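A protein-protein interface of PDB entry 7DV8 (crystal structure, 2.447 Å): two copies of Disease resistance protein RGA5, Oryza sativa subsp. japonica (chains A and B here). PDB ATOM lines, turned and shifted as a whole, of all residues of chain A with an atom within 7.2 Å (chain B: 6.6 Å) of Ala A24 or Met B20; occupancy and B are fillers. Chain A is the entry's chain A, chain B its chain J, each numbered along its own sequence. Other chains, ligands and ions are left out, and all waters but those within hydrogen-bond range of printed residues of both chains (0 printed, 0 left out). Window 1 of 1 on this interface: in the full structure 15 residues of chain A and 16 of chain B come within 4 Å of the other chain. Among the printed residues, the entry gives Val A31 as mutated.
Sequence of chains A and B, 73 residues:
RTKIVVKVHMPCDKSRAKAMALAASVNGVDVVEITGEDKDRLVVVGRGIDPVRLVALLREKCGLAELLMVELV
Met A20 touches Ala B24, and with the chains exchanged Ala A24 touches Met B20.
Ala B21 touches its own counterpart, Ala A21.
Ala A21 touches Ala B24, and with the chains exchanged Ala A24 touches Ala B21.
Ser A25 touches Ala B21, but with the chains exchanged Ala A21 does not touch Ser B25 (4.2 Å).
10 positions are printed for both chains.
Hydrophobic or aromatic side chains of chain A within 4 Å of the printed part of chain B: Met A20, Ala A21, Ala A24, Val A29, Val A31 and Val A32.
Of the 18 printed residues of chain B, 8 touch a printed residue of chain A.
Among the printed residues, 18 pairs touch across the chains.
Among the printed residues, Asp or Glu carboxylates within 4 Å of a Lys or Arg side-chain nitrogen of the other chain: Asp A30 with Arg B16.
The guanidinium group of Arg B16 lies within salt-bridge range of the side-chain carboxylate of Asp A30.
The backbone carbonyl oxygen (O) of Asp A30 lies within hydrogen-bond range of the backbone NH (N) of Ile B34 (3.3 Å).
O of Val B32 sits at hydrogen-bond distance from N of Val A32.
The side-chain sulfur of Met B20 lies close to the backbone carbonyl oxygen of Val A29.
C of Met A20 touches CB of Ala B24, at 3.6 Å.
Ala A24 touches Ala B17.
C of Met B20 touches CB of Ala A24, 3.7 Å away.
Ser A25 touches Ala B17.
Asn A27 touches Ala B17 (OD1 to CB, 3.7 Å).
O of Val A29 touches NH1 of Arg B16, at 3.98 Å.
Asp A30 touches Met B20 (O to SD, 3.8 Å).
Asp A30 touches Glu B33 (O to CA, 3.2 Å).
CA of Val A31 touches O of Val B32 (3.4 Å).
Glu B33 touches Val A31.
OG of Ser A25 lies close to O of Ala A21, at 3.4 Å.
The backbone carbonyl oxygen of Leu A22 lies within hydrogen-bond range of the side-chain hydroxyl of Ser A25.
The backbone carbonyl oxygen (O) of Val A45 is in hydrogen-bond range of the backbone NH (N) of Asp A30, at 2.8 Å.
N of Val A45 lies within hydrogen-bond range of O of Val A31 (2.9 Å).
Leu A22 touches none of the printed residues of chain B.
Ala A24 touches three residues of chain B.
Printed residues of chain B within 4 Å of Asn A27: Ala B17 (3.7 Å).
Val A45 touches none of the printed residues of chain B.
Of the printed residues of chain A, Ala B17 touches Ala A24, Ser A25 and Asn A27.
No residue of chain A comes within 4 Å of Ala B19.
Of chain A, only Ala A24, Val A29 and Asp A30 come within 4 Å of Met B20.
The nearest residue of chain B that does not touch Ala A24 is Ala B24 (4.1 Å).
The nearest printed residue of chain A that does not touch Ala B17 is Val A26 (4.6 Å).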
ATOM      1  N   LYS A  18      24.613  28.370  12.242  1.00  0.00           N
ATOM      2  CA  LYS A  18      23.284  28.066  11.743  1.00  0.00           C
ATOM      3  C   LYS A  18      22.905  26.607  11.976  1.00  0.00           C
ATOM      4  O   LYS A  18      21.722  26.309  12.190  1.00  0.00           O
ATOM      5  CB  LYS A  18      23.189  28.437  10.274  1.00  0.00           C
ATOM      6  CG  LYS A  18      23.331  29.927  10.096  1.00  0.00           C
ATOM      7  CD  LYS A  18      22.497  30.358   8.919  1.00  0.00           C
ATOM      8  CE  LYS A  18      23.177  30.027   7.593  1.00  0.00           C
ATOM      9  NZ  LYS A  18      23.279  31.184   6.666  1.00  0.00           N
ATOM     10  N   ALA A  19      23.891  25.697  11.989  1.00  0.00           N
ATOM     11  CA  ALA A  19      23.608  24.304  12.314  1.00  0.00           C
ATOM     12  C   ALA A  19      23.402  24.129  13.815  1.00  0.00           C
ATOM     13  O   ALA A  19      22.495  23.396  14.244  1.00  0.00           O
ATOM     14  CB  ALA A  19      24.737  23.398  11.813  1.00  0.00           C
ATOM     15  N   MET A  20      24.249  24.782  14.616  1.00  0.00           N
ATOM     16  CA  MET A  20      24.080  24.752  16.062  1.00  0.00           C
ATOM     17  C   MET A  20      22.712  25.277  16.451  1.00  0.00           C
ATOM     18  O   MET A  20      21.996  24.645  17.234  1.00  0.00           O
ATOM     19  CB  MET A  20      25.181  25.570  16.733  1.00  0.00           C
ATOM     20  CG  MET A  20      26.550  24.911  16.633  1.00  0.00           C
ATOM     21  SD  MET A  20      26.822  23.757  17.991  1.00  0.00           S
ATOM     22  CE  MET A  20      27.082  24.960  19.323  1.00  0.00           C
ATOM     23  N   ALA A  21      22.305  26.406  15.871  1.00  0.00           N
ATOM     24  CA  ALA A  21      21.022  26.985  16.256  1.00  0.00           C
ATOM     25  C   ALA A  21      19.860  26.138  15.750  1.00  0.00           C
ATOM     26  O   ALA A  21      18.830  26.044  16.430  1.00  0.00           O
ATOM     27  CB  ALA A  21      20.911  28.432  15.761  1.00  0.00           C
ATOM     28  N   LEU A  22      20.009  25.503  14.581  1.00  0.00           N
ATOM     29  CA  LEU A  22      18.946  24.635  14.087  1.00  0.00           C
ATOM     30  C   LEU A  22      18.724  23.458  15.030  1.00  0.00           C
ATOM     31  O   LEU A  22      17.596  23.213  15.475  1.00  0.00           O
ATOM     32  CB  LEU A  22      19.266  24.144  12.678  1.00  0.00           C
ATOM     33  CG  LEU A  22      18.013  23.926  11.828  1.00  0.00           C
ATOM     34  CD1 LEU A  22      17.394  25.266  11.461  1.00  0.00           C
ATOM     35  CD2 LEU A  22      18.345  23.128  10.579  1.00  0.00           C
ATOM     36  N   ALA A  23      19.796  22.726  15.352  1.00  0.00           N
ATOM     37  CA  ALA A  23      19.698  21.644  16.325  1.00  0.00           C
ATOM     38  C   ALA A  23      19.133  22.142  17.655  1.00  0.00           C
ATOM     39  O   ALA A  23      18.230  21.518  18.234  1.00  0.00           O
ATOM     40  CB  ALA A  23      21.069  21.004  16.531  1.00  0.00           C
ATOM     41  N   ALA A  24      19.654  23.276  18.144  1.00  0.00           N
ATOM     42  CA  ALA A  24      19.218  23.831  19.419  1.00  0.00           C
ATOM     43  C   ALA A  24      17.718  24.110  19.437  1.00  0.00           C
ATOM     44  O   ALA A  24      17.048  23.892  20.454  1.00  0.00           O
ATOM     45  CB  ALA A  24      20.004  25.111  19.719  1.00  0.00           C
ATOM     46  N   SER A  25      17.166  24.583  18.321  1.00  0.00           N
ATOM     47  CA  SER A  25      15.762  24.974  18.314  1.00  0.00           C
ATOM     48  C   SER A  25      14.805  23.782  18.364  1.00  0.00           C
ATOM     49  O   SER A  25      13.590  24.005  18.440  1.00  0.00           O
ATOM     50  CB  SER A  25      15.476  25.833  17.078  1.00  0.00           C
ATOM     51  OG  SER A  25      15.565  25.070  15.889  1.00  0.00           O
ATOM     52  N   VAL A  26      15.311  22.543  18.333  1.00  0.00           N
ATOM     53  CA  VAL A  26      14.467  21.347  18.408  1.00  0.00           C
ATOM     54  C   VAL A  26      14.121  21.040  19.864  1.00  0.00           C
ATOM     55  O   VAL A  26      15.011  20.805  20.697  1.00  0.00           O
ATOM     56  CB  VAL A  26      15.136  20.133  17.744  1.00  0.00           C
ATOM     57  CG1 VAL A  26      14.237  18.889  17.930  1.00  0.00           C
ATOM     58  CG2 VAL A  26      15.380  20.392  16.273  1.00  0.00           C
ATOM     59  N   ASN A  27      12.818  20.959  20.150  1.00  0.00           N
ATOM     60  CA  ASN A  27      12.373  20.831  21.531  1.00  0.00           C
ATOM     61  C   ASN A  27      12.824  19.498  22.106  1.00  0.00           C
ATOM     62  O   ASN A  27      12.685  18.444  21.480  1.00  0.00           O
ATOM     63  CB  ASN A  27      10.847  20.991  21.630  1.00  0.00           C
ATOM     64  CG  ASN A  27      10.407  22.431  21.444  1.00  0.00           C
ATOM     65  OD1 ASN A  27      11.133  23.231  20.847  1.00  0.00           O
ATOM     66  ND2 ASN A  27       9.223  22.769  21.936  1.00  0.00           N
ATOM     67  N   GLY A  28      13.372  19.557  23.303  1.00  0.00           N
ATOM     68  CA  GLY A  28      13.967  18.394  23.896  1.00  0.00           C
ATOM     69  C   GLY A  28      15.465  18.319  23.750  1.00  0.00           C
ATOM     70  O   GLY A  28      16.092  17.499  24.423  1.00  0.00           O
ATOM     71  N   VAL A  29      16.062  19.139  22.898  1.00  0.00           N
ATOM     72  CA  VAL A  29      17.510  19.124  22.759  1.00  0.00           C
ATOM     73  C   VAL A  29      18.136  19.827  23.949  1.00  0.00           C
ATOM     74  O   VAL A  29      17.785  20.969  24.264  1.00  0.00           O
ATOM     75  CB  VAL A  29      17.945  19.776  21.445  1.00  0.00           C
ATOM     76  CG1 VAL A  29      19.420  20.180  21.495  1.00  0.00           C
ATOM     77  CG2 VAL A  29      17.674  18.809  20.307  1.00  0.00           C
ATOM     78  N   ASP A  30      19.088  19.147  24.586  1.00  0.00           N
ATOM     79  CA  ASP A  30      19.807  19.589  25.774  1.00  0.00           C
ATOM     80  C   ASP A  30      21.262  19.949  25.493  1.00  0.00           C
ATOM     81  O   ASP A  30      21.852  20.710  26.262  1.00  0.00           O
ATOM     82  CB  ASP A  30      19.788  18.493  26.846  1.00  0.00           C
ATOM     83  CG  ASP A  30      18.380  17.963  27.142  1.00  0.00           C
ATOM     84  OD1 ASP A  30      17.400  18.716  26.936  1.00  0.00           O
ATOM     85  OD2 ASP A  30      18.283  16.786  27.615  1.00  0.00           O
ATOM     86  N   VAL A  31      21.883  19.388  24.454  1.00  0.00           N
ATOM     87  CA  VAL A  31      23.293  19.654  24.155  1.00  0.00           C
ATOM     88  C   VAL A  31      23.490  19.735  22.647  1.00  0.00           C
ATOM     89  O   VAL A  31      23.086  18.828  21.911  1.00  0.00           O
ATOM     90  CB  VAL A  31      24.239  18.574  24.720  1.00  0.00           C
ATOM     91  CG1 VAL A  31      25.665  18.869  24.296  1.00  0.00           C
ATOM     92  CG2 VAL A  31      24.149  18.477  26.208  1.00  0.00           C
ATOM     93  N   VAL A  32      24.132  20.804  22.191  1.00  0.00           N
ATOM     94  CA  VAL A  32      24.610  20.908  20.819  1.00  0.00           C
ATOM     95  C   VAL A  32      26.105  21.201  20.883  1.00  0.00           C
ATOM     96  O   VAL A  32      26.547  22.054  21.665  1.00  0.00           O
ATOM     97  CB  VAL A  32      23.846  21.985  20.022  1.00  0.00           C
ATOM     98  CG1 VAL A  32      22.345  21.637  19.961  1.00  0.00           C
ATOM     99  CG2 VAL A  32      24.016  23.353  20.663  1.00  0.00           C
ATOM    100  N   LEU A  42      28.492  17.659  14.124  1.00  0.00           N
ATOM    101  CA  LEU A  42      27.506  18.202  15.040  1.00  0.00           C
ATOM    102  C   LEU A  42      27.049  17.077  15.958  1.00  0.00           C
ATOM    103  O   LEU A  42      26.544  16.050  15.487  1.00  0.00           O
ATOM    104  CB  LEU A  42      26.326  18.818  14.283  1.00  0.00           C
ATOM    105  CG  LEU A  42      25.276  19.570  15.125  1.00  0.00           C
ATOM    106  CD1 LEU A  42      25.796  20.923  15.630  1.00  0.00           C
ATOM    107  CD2 LEU A  42      23.987  19.740  14.331  1.00  0.00           C
ATOM    108  N   VAL A  44      24.476  16.168  18.957  1.00  0.00           N
ATOM    109  CA  VAL A  44      23.185  16.615  19.466  1.00  0.00           C
ATOM    110  C   VAL A  44      22.671  15.569  20.447  1.00  0.00           C
ATOM    111  O   VAL A  44      22.564  14.384  20.099  1.00  0.00           O
ATOM    112  CB  VAL A  44      22.160  16.853  18.343  1.00  0.00           C
ATOM    113  CG1 VAL A  44      20.825  17.381  18.931  1.00  0.00           C
ATOM    114  CG2 VAL A  44      22.708  17.830  17.296  1.00  0.00           C
ATOM    115  N   VAL A  45      22.340  16.011  21.666  1.00  0.00           N
ATOM    116  CA  VAL A  45      21.814  15.150  22.723  1.00  0.00           C
ATOM    117  C   VAL A  45      20.481  15.714  23.218  1.00  0.00           C
ATOM    118  O   VAL A  45      20.306  16.938  23.282  1.00  0.00           O
ATOM    119  CB  VAL A  45      22.830  15.020  23.878  1.00  0.00           C
ATOM    120  CG1 VAL A  45      22.389  13.972  24.872  1.00  0.00           C
ATOM    121  CG2 VAL A  45      24.226  14.716  23.331  1.00  0.00           C
ATOM    122  N   LEU A  54      15.858  15.421  11.870  1.00  0.00           N
ATOM    123  CA  LEU A  54      16.954  16.321  12.195  1.00  0.00           C
ATOM    124  C   LEU A  54      17.917  16.453  11.022  1.00  0.00           C
ATOM    125  O   LEU A  54      18.250  17.569  10.597  1.00  0.00           O
ATOM    126  CB  LEU A  54      17.697  15.809  13.424  1.00  0.00           C
ATOM    127  CG  LEU A  54      18.866  16.681  13.878  1.00  0.00           C
ATOM    128  CD1 LEU A  54      18.372  18.041  14.386  1.00  0.00           C
ATOM    129  CD2 LEU A  54      19.705  15.951  14.924  1.00  0.00           C
ATOM    130  N   MET B  10      13.618  29.369  32.118  1.00  0.00           N
ATOM    131  CA  MET B  10      13.260  28.509  30.990  1.00  0.00           C
ATOM    132  C   MET B  10      12.369  27.405  31.526  1.00  0.00           C
ATOM    133  O   MET B  10      12.730  26.230  31.511  1.00  0.00           O
ATOM    134  CB  MET B  10      14.505  27.933  30.314  1.00  0.00           C
ATOM    135  CG  MET B  10      15.610  28.936  30.022  1.00  0.00           C
ATOM    136  SD  MET B  10      17.108  28.194  29.324  1.00  0.00           S
ATOM    137  CE  MET B  10      17.814  27.285  30.694  1.00  0.00           C
ATOM    138  N   SER B  15      10.780  27.407  25.454  1.00  0.00           N
ATOM    139  CA  SER B  15      11.606  28.504  25.945  1.00  0.00           C
ATOM    140  C   SER B  15      13.055  28.079  26.184  1.00  0.00           C
ATOM    141  O   SER B  15      13.968  28.893  25.993  1.00  0.00           O
ATOM    142  CB  SER B  15      10.997  29.104  27.224  1.00  0.00           C
ATOM    143  OG  SER B  15      11.453  28.462  28.407  1.00  0.00           O
ATOM    144  N   ARG B  16      13.293  26.834  26.612  1.00  0.00           N
ATOM    145  CA  ARG B  16      14.673  26.372  26.748  1.00  0.00           C
ATOM    146  C   ARG B  16      15.340  26.197  25.374  1.00  0.00           C
ATOM    147  O   ARG B  16      16.535  26.493  25.217  1.00  0.00           O
ATOM    148  CB  ARG B  16      14.735  25.075  27.564  1.00  0.00           C
ATOM    149  CG  ARG B  16      14.207  23.859  26.833  1.00  0.00           C
ATOM    150  CD  ARG B  16      13.914  22.683  27.766  1.00  0.00           C
ATOM    151  NE  ARG B  16      14.900  22.493  28.829  1.00  0.00           N
ATOM    152  CZ  ARG B  16      15.833  21.540  28.803  1.00  0.00           C
ATOM    153  NH1 ARG B  16      15.909  20.703  27.765  1.00  0.00           N
ATOM    154  NH2 ARG B  16      16.695  21.423  29.809  1.00  0.00           N
ATOM    155  N   ALA B  17      14.574  25.783  24.363  1.00  0.00           N
ATOM    156  CA  ALA B  17      15.079  25.814  22.997  1.00  0.00           C
ATOM    157  C   ALA B  17      15.298  27.241  22.497  1.00  0.00           C
ATOM    158  O   ALA B  17      16.181  27.473  21.659  1.00  0.00           O
ATOM    159  CB  ALA B  17      14.126  25.069  22.062  1.00  0.00           C
ATOM    160  N   LYS B  18      14.503  28.201  22.977  1.00  0.00           N
ATOM    161  CA  LYS B  18      14.666  29.582  22.534  1.00  0.00           C
ATOM    162  C   LYS B  18      16.016  30.128  22.966  1.00  0.00           C
ATOM    163  O   LYS B  18      16.791  30.634  22.140  1.00  0.00           O
ATOM    164  CB  LYS B  18      13.537  30.452  23.078  1.00  0.00           C
ATOM    165  CG  LYS B  18      13.106  31.598  22.169  1.00  0.00           C
ATOM    166  CD  LYS B  18      12.186  32.564  22.926  1.00  0.00           C
ATOM    167  CE  LYS B  18      11.380  33.469  21.992  1.00  0.00           C
ATOM    168  NZ  LYS B  18      10.512  34.415  22.752  1.00  0.00           N
ATOM    169  N   ALA B  19      16.322  30.012  24.262  1.00  0.00           N
ATOM    170  CA  ALA B  19      17.617  30.454  24.772  1.00  0.00           C
ATOM    171  C   ALA B  19      18.767  29.695  24.112  1.00  0.00           C
ATOM    172  O   ALA B  19      19.775  30.292  23.711  1.00  0.00           O
ATOM    173  CB  ALA B  19      17.668  30.283  26.287  1.00  0.00           C
ATOM    174  N   MET B  20      18.642  28.370  24.015  1.00  0.00           N
ATOM    175  CA  MET B  20      19.711  27.574  23.425  1.00  0.00           C
ATOM    176  C   MET B  20      20.004  28.017  21.998  1.00  0.00           C
ATOM    177  O   MET B  20      21.162  28.252  21.642  1.00  0.00           O
ATOM    178  CB  MET B  20      19.359  26.090  23.472  1.00  0.00           C
ATOM    179  CG  MET B  20      19.562  25.463  24.828  1.00  0.00           C
ATOM    180  SD  MET B  20      20.183  23.772  24.719  1.00  0.00           S
ATOM    181  CE  MET B  20      19.691  23.330  23.062  1.00  0.00           C
ATOM    182  N   ALA B  21      18.959  28.163  21.177  1.00  0.00           N
ATOM    183  CA  ALA B  21      19.168  28.543  19.786  1.00  0.00           C
ATOM    184  C   ALA B  21      19.764  29.946  19.675  1.00  0.00           C
ATOM    185  O   ALA B  21      20.617  30.196  18.807  1.00  0.00           O
ATOM    186  CB  ALA B  21      17.857  28.433  19.005  1.00  0.00           C
ATOM    187  N   LEU B  22      19.373  30.858  20.566  1.00  0.00           N
ATOM    188  CA  LEU B  22      19.923  32.201  20.472  1.00  0.00           C
ATOM    189  C   LEU B  22      21.401  32.224  20.858  1.00  0.00           C
ATOM    190  O   LEU B  22      22.203  32.898  20.200  1.00  0.00           O
ATOM    191  CB  LEU B  22      19.111  33.170  21.330  1.00  0.00           C
ATOM    192  CG  LEU B  22      19.619  34.598  21.150  1.00  0.00           C
ATOM    193  CD1 LEU B  22      18.475  35.529  20.812  1.00  0.00           C
ATOM    194  CD2 LEU B  22      20.378  35.082  22.380  1.00  0.00           C
ATOM    195  N   ALA B  23      21.796  31.485  21.902  1.00  0.00           N
ATOM    196  CA  ALA B  23      23.220  31.416  22.231  1.00  0.00           C
ATOM    197  C   ALA B  23      23.995  30.698  21.135  1.00  0.00           C
ATOM    198  O   ALA B  23      25.102  31.118  20.773  1.00  0.00           O
ATOM    199  CB  ALA B  23      23.436  30.719  23.573  1.00  0.00           C
ATOM    200  N   ALA B  24      23.417  29.617  20.594  1.00  0.00           N
ATOM    201  CA  ALA B  24      24.058  28.863  19.524  1.00  0.00           C
ATOM    202  C   ALA B  24      24.318  29.728  18.296  1.00  0.00           C
ATOM    203  O   ALA B  24      25.264  29.480  17.551  1.00  0.00           O
ATOM    204  CB  ALA B  24      23.187  27.669  19.140  1.00  0.00           C
ATOM    205  N   SER B  25      23.488  30.742  18.072  1.00  0.00           N
ATOM    206  CA  SER B  25      23.606  31.557  16.875  1.00  0.00           C
ATOM    207  C   SER B  25      24.781  32.532  16.927  1.00  0.00           C
ATOM    208  O   SER B  25      25.061  33.184  15.914  1.00  0.00           O
ATOM    209  CB  SER B  25      22.291  32.306  16.653  1.00  0.00           C
ATOM    210  OG  SER B  25      22.149  33.343  17.594  1.00  0.00           O
ATOM    211  N   VAL B  32      26.824  24.436  23.553  1.00  0.00           N
ATOM    212  CA  VAL B  32      25.671  24.963  24.271  1.00  0.00           C
ATOM    213  C   VAL B  32      25.025  23.791  24.999  1.00  0.00           C
ATOM    214  O   VAL B  32      24.801  22.737  24.390  1.00  0.00           O
ATOM    215  CB  VAL B  32      24.667  25.648  23.321  1.00  0.00           C
ATOM    216  CG1 VAL B  32      23.534  26.259  24.101  1.00  0.00           C
ATOM    217  CG2 VAL B  32      25.362  26.724  22.491  1.00  0.00           C
ATOM    218  N   GLU B  33      24.763  23.956  26.304  1.00  0.00           N
ATOM    219  CA  GLU B  33      24.072  22.929  27.079  1.00  0.00           C
ATOM    220  C   GLU B  33      23.366  23.544  28.279  1.00  0.00           C
ATOM    221  O   GLU B  33      23.826  24.530  28.860  1.00  0.00           O
ATOM    222  CB  GLU B  33      25.017  21.817  27.559  1.00  0.00           C
ATOM    223  CG  GLU B  33      26.339  22.282  28.114  1.00  0.00           C
ATOM    224  CD  GLU B  33      27.219  21.130  28.576  1.00  0.00           C
ATOM    225  OE1 GLU B  33      26.720  19.985  28.616  1.00  0.00           O
ATOM    226  OE2 GLU B  33      28.405  21.368  28.904  1.00  0.00           O
ATOM    227  N   ILE B  34      22.235  22.945  28.639  1.00  0.00           N
ATOM    228  CA  ILE B  34      21.460  23.334  29.811  1.00  0.00           C
ATOM    229  C   ILE B  34      21.701  22.302  30.907  1.00  0.00           C
ATOM    230  O   ILE B  34      21.561  21.096  30.671  1.00  0.00           O
ATOM    231  CB  ILE B  34      19.963  23.453  29.464  1.00  0.00           C
ATOM    232  CG1 ILE B  34      19.719  24.709  28.617  1.00  0.00           C
ATOM    233  CG2 ILE B  34      19.093  23.449  30.722  1.00  0.00           C
ATOM    234  CD1 ILE B  34      18.323  24.776  28.030  1.00  0.00           C
ATOM    235  N   LEU B  42      22.347  27.749  31.609  1.00  0.00           N
ATOM    236  CA  LEU B  42      22.791  27.759  30.226  1.00  0.00           C
ATOM    237  C   LEU B  42      24.300  27.974  30.220  1.00  0.00           C
ATOM    238  O   LEU B  42      24.786  29.010  30.700  1.00  0.00           O
ATOM    239  CB  LEU B  42      22.093  28.875  29.448  1.00  0.00           C
ATOM    240  CG  LEU B  42      22.368  28.936  27.942  1.00  0.00           C
ATOM    241  CD1 LEU B  42      21.906  27.664  27.185  1.00  0.00           C
ATOM    242  CD2 LEU B  42      21.805  30.216  27.328  1.00  0.00           C
ATOM    243  N   LEU B  58      19.922  37.595  25.567  1.00  0.00           N
ATOM    244  CA  LEU B  58      19.070  36.705  26.348  1.00  0.00           C
ATOM    245  C   LEU B  58      17.987  37.489  27.076  1.00  0.00           C
ATOM    246  O   LEU B  58      16.806  37.120  27.033  1.00  0.00           O
ATOM    247  CB  LEU B  58      19.916  35.907  27.338  1.00  0.00           C
ATOM    248  CG  LEU B  58      20.788  34.827  26.697  1.00  0.00           C
ATOM    249  CD1 LEU B  58      21.896  34.401  27.648  1.00  0.00           C
ATOM    250  CD2 LEU B  58      19.913  33.639  26.307  1.00  0.00           C
ATOM    251  N   CYS B  62      14.220  36.658  26.082  1.00  0.00           N
ATOM    252  CA  CYS B  62      13.742  35.566  26.918  1.00  0.00           C
ATOM    253  C   CYS B  62      13.086  36.065  28.191  1.00  0.00           C
ATOM    254  O   CYS B  62      11.862  36.193  28.248  1.00  0.00           O
ATOM    255  CB  CYS B  62      14.891  34.632  27.270  1.00  0.00           C
ATOM    256  SG  CYS B  62      15.482  33.711  25.843  1.00  0.00           S
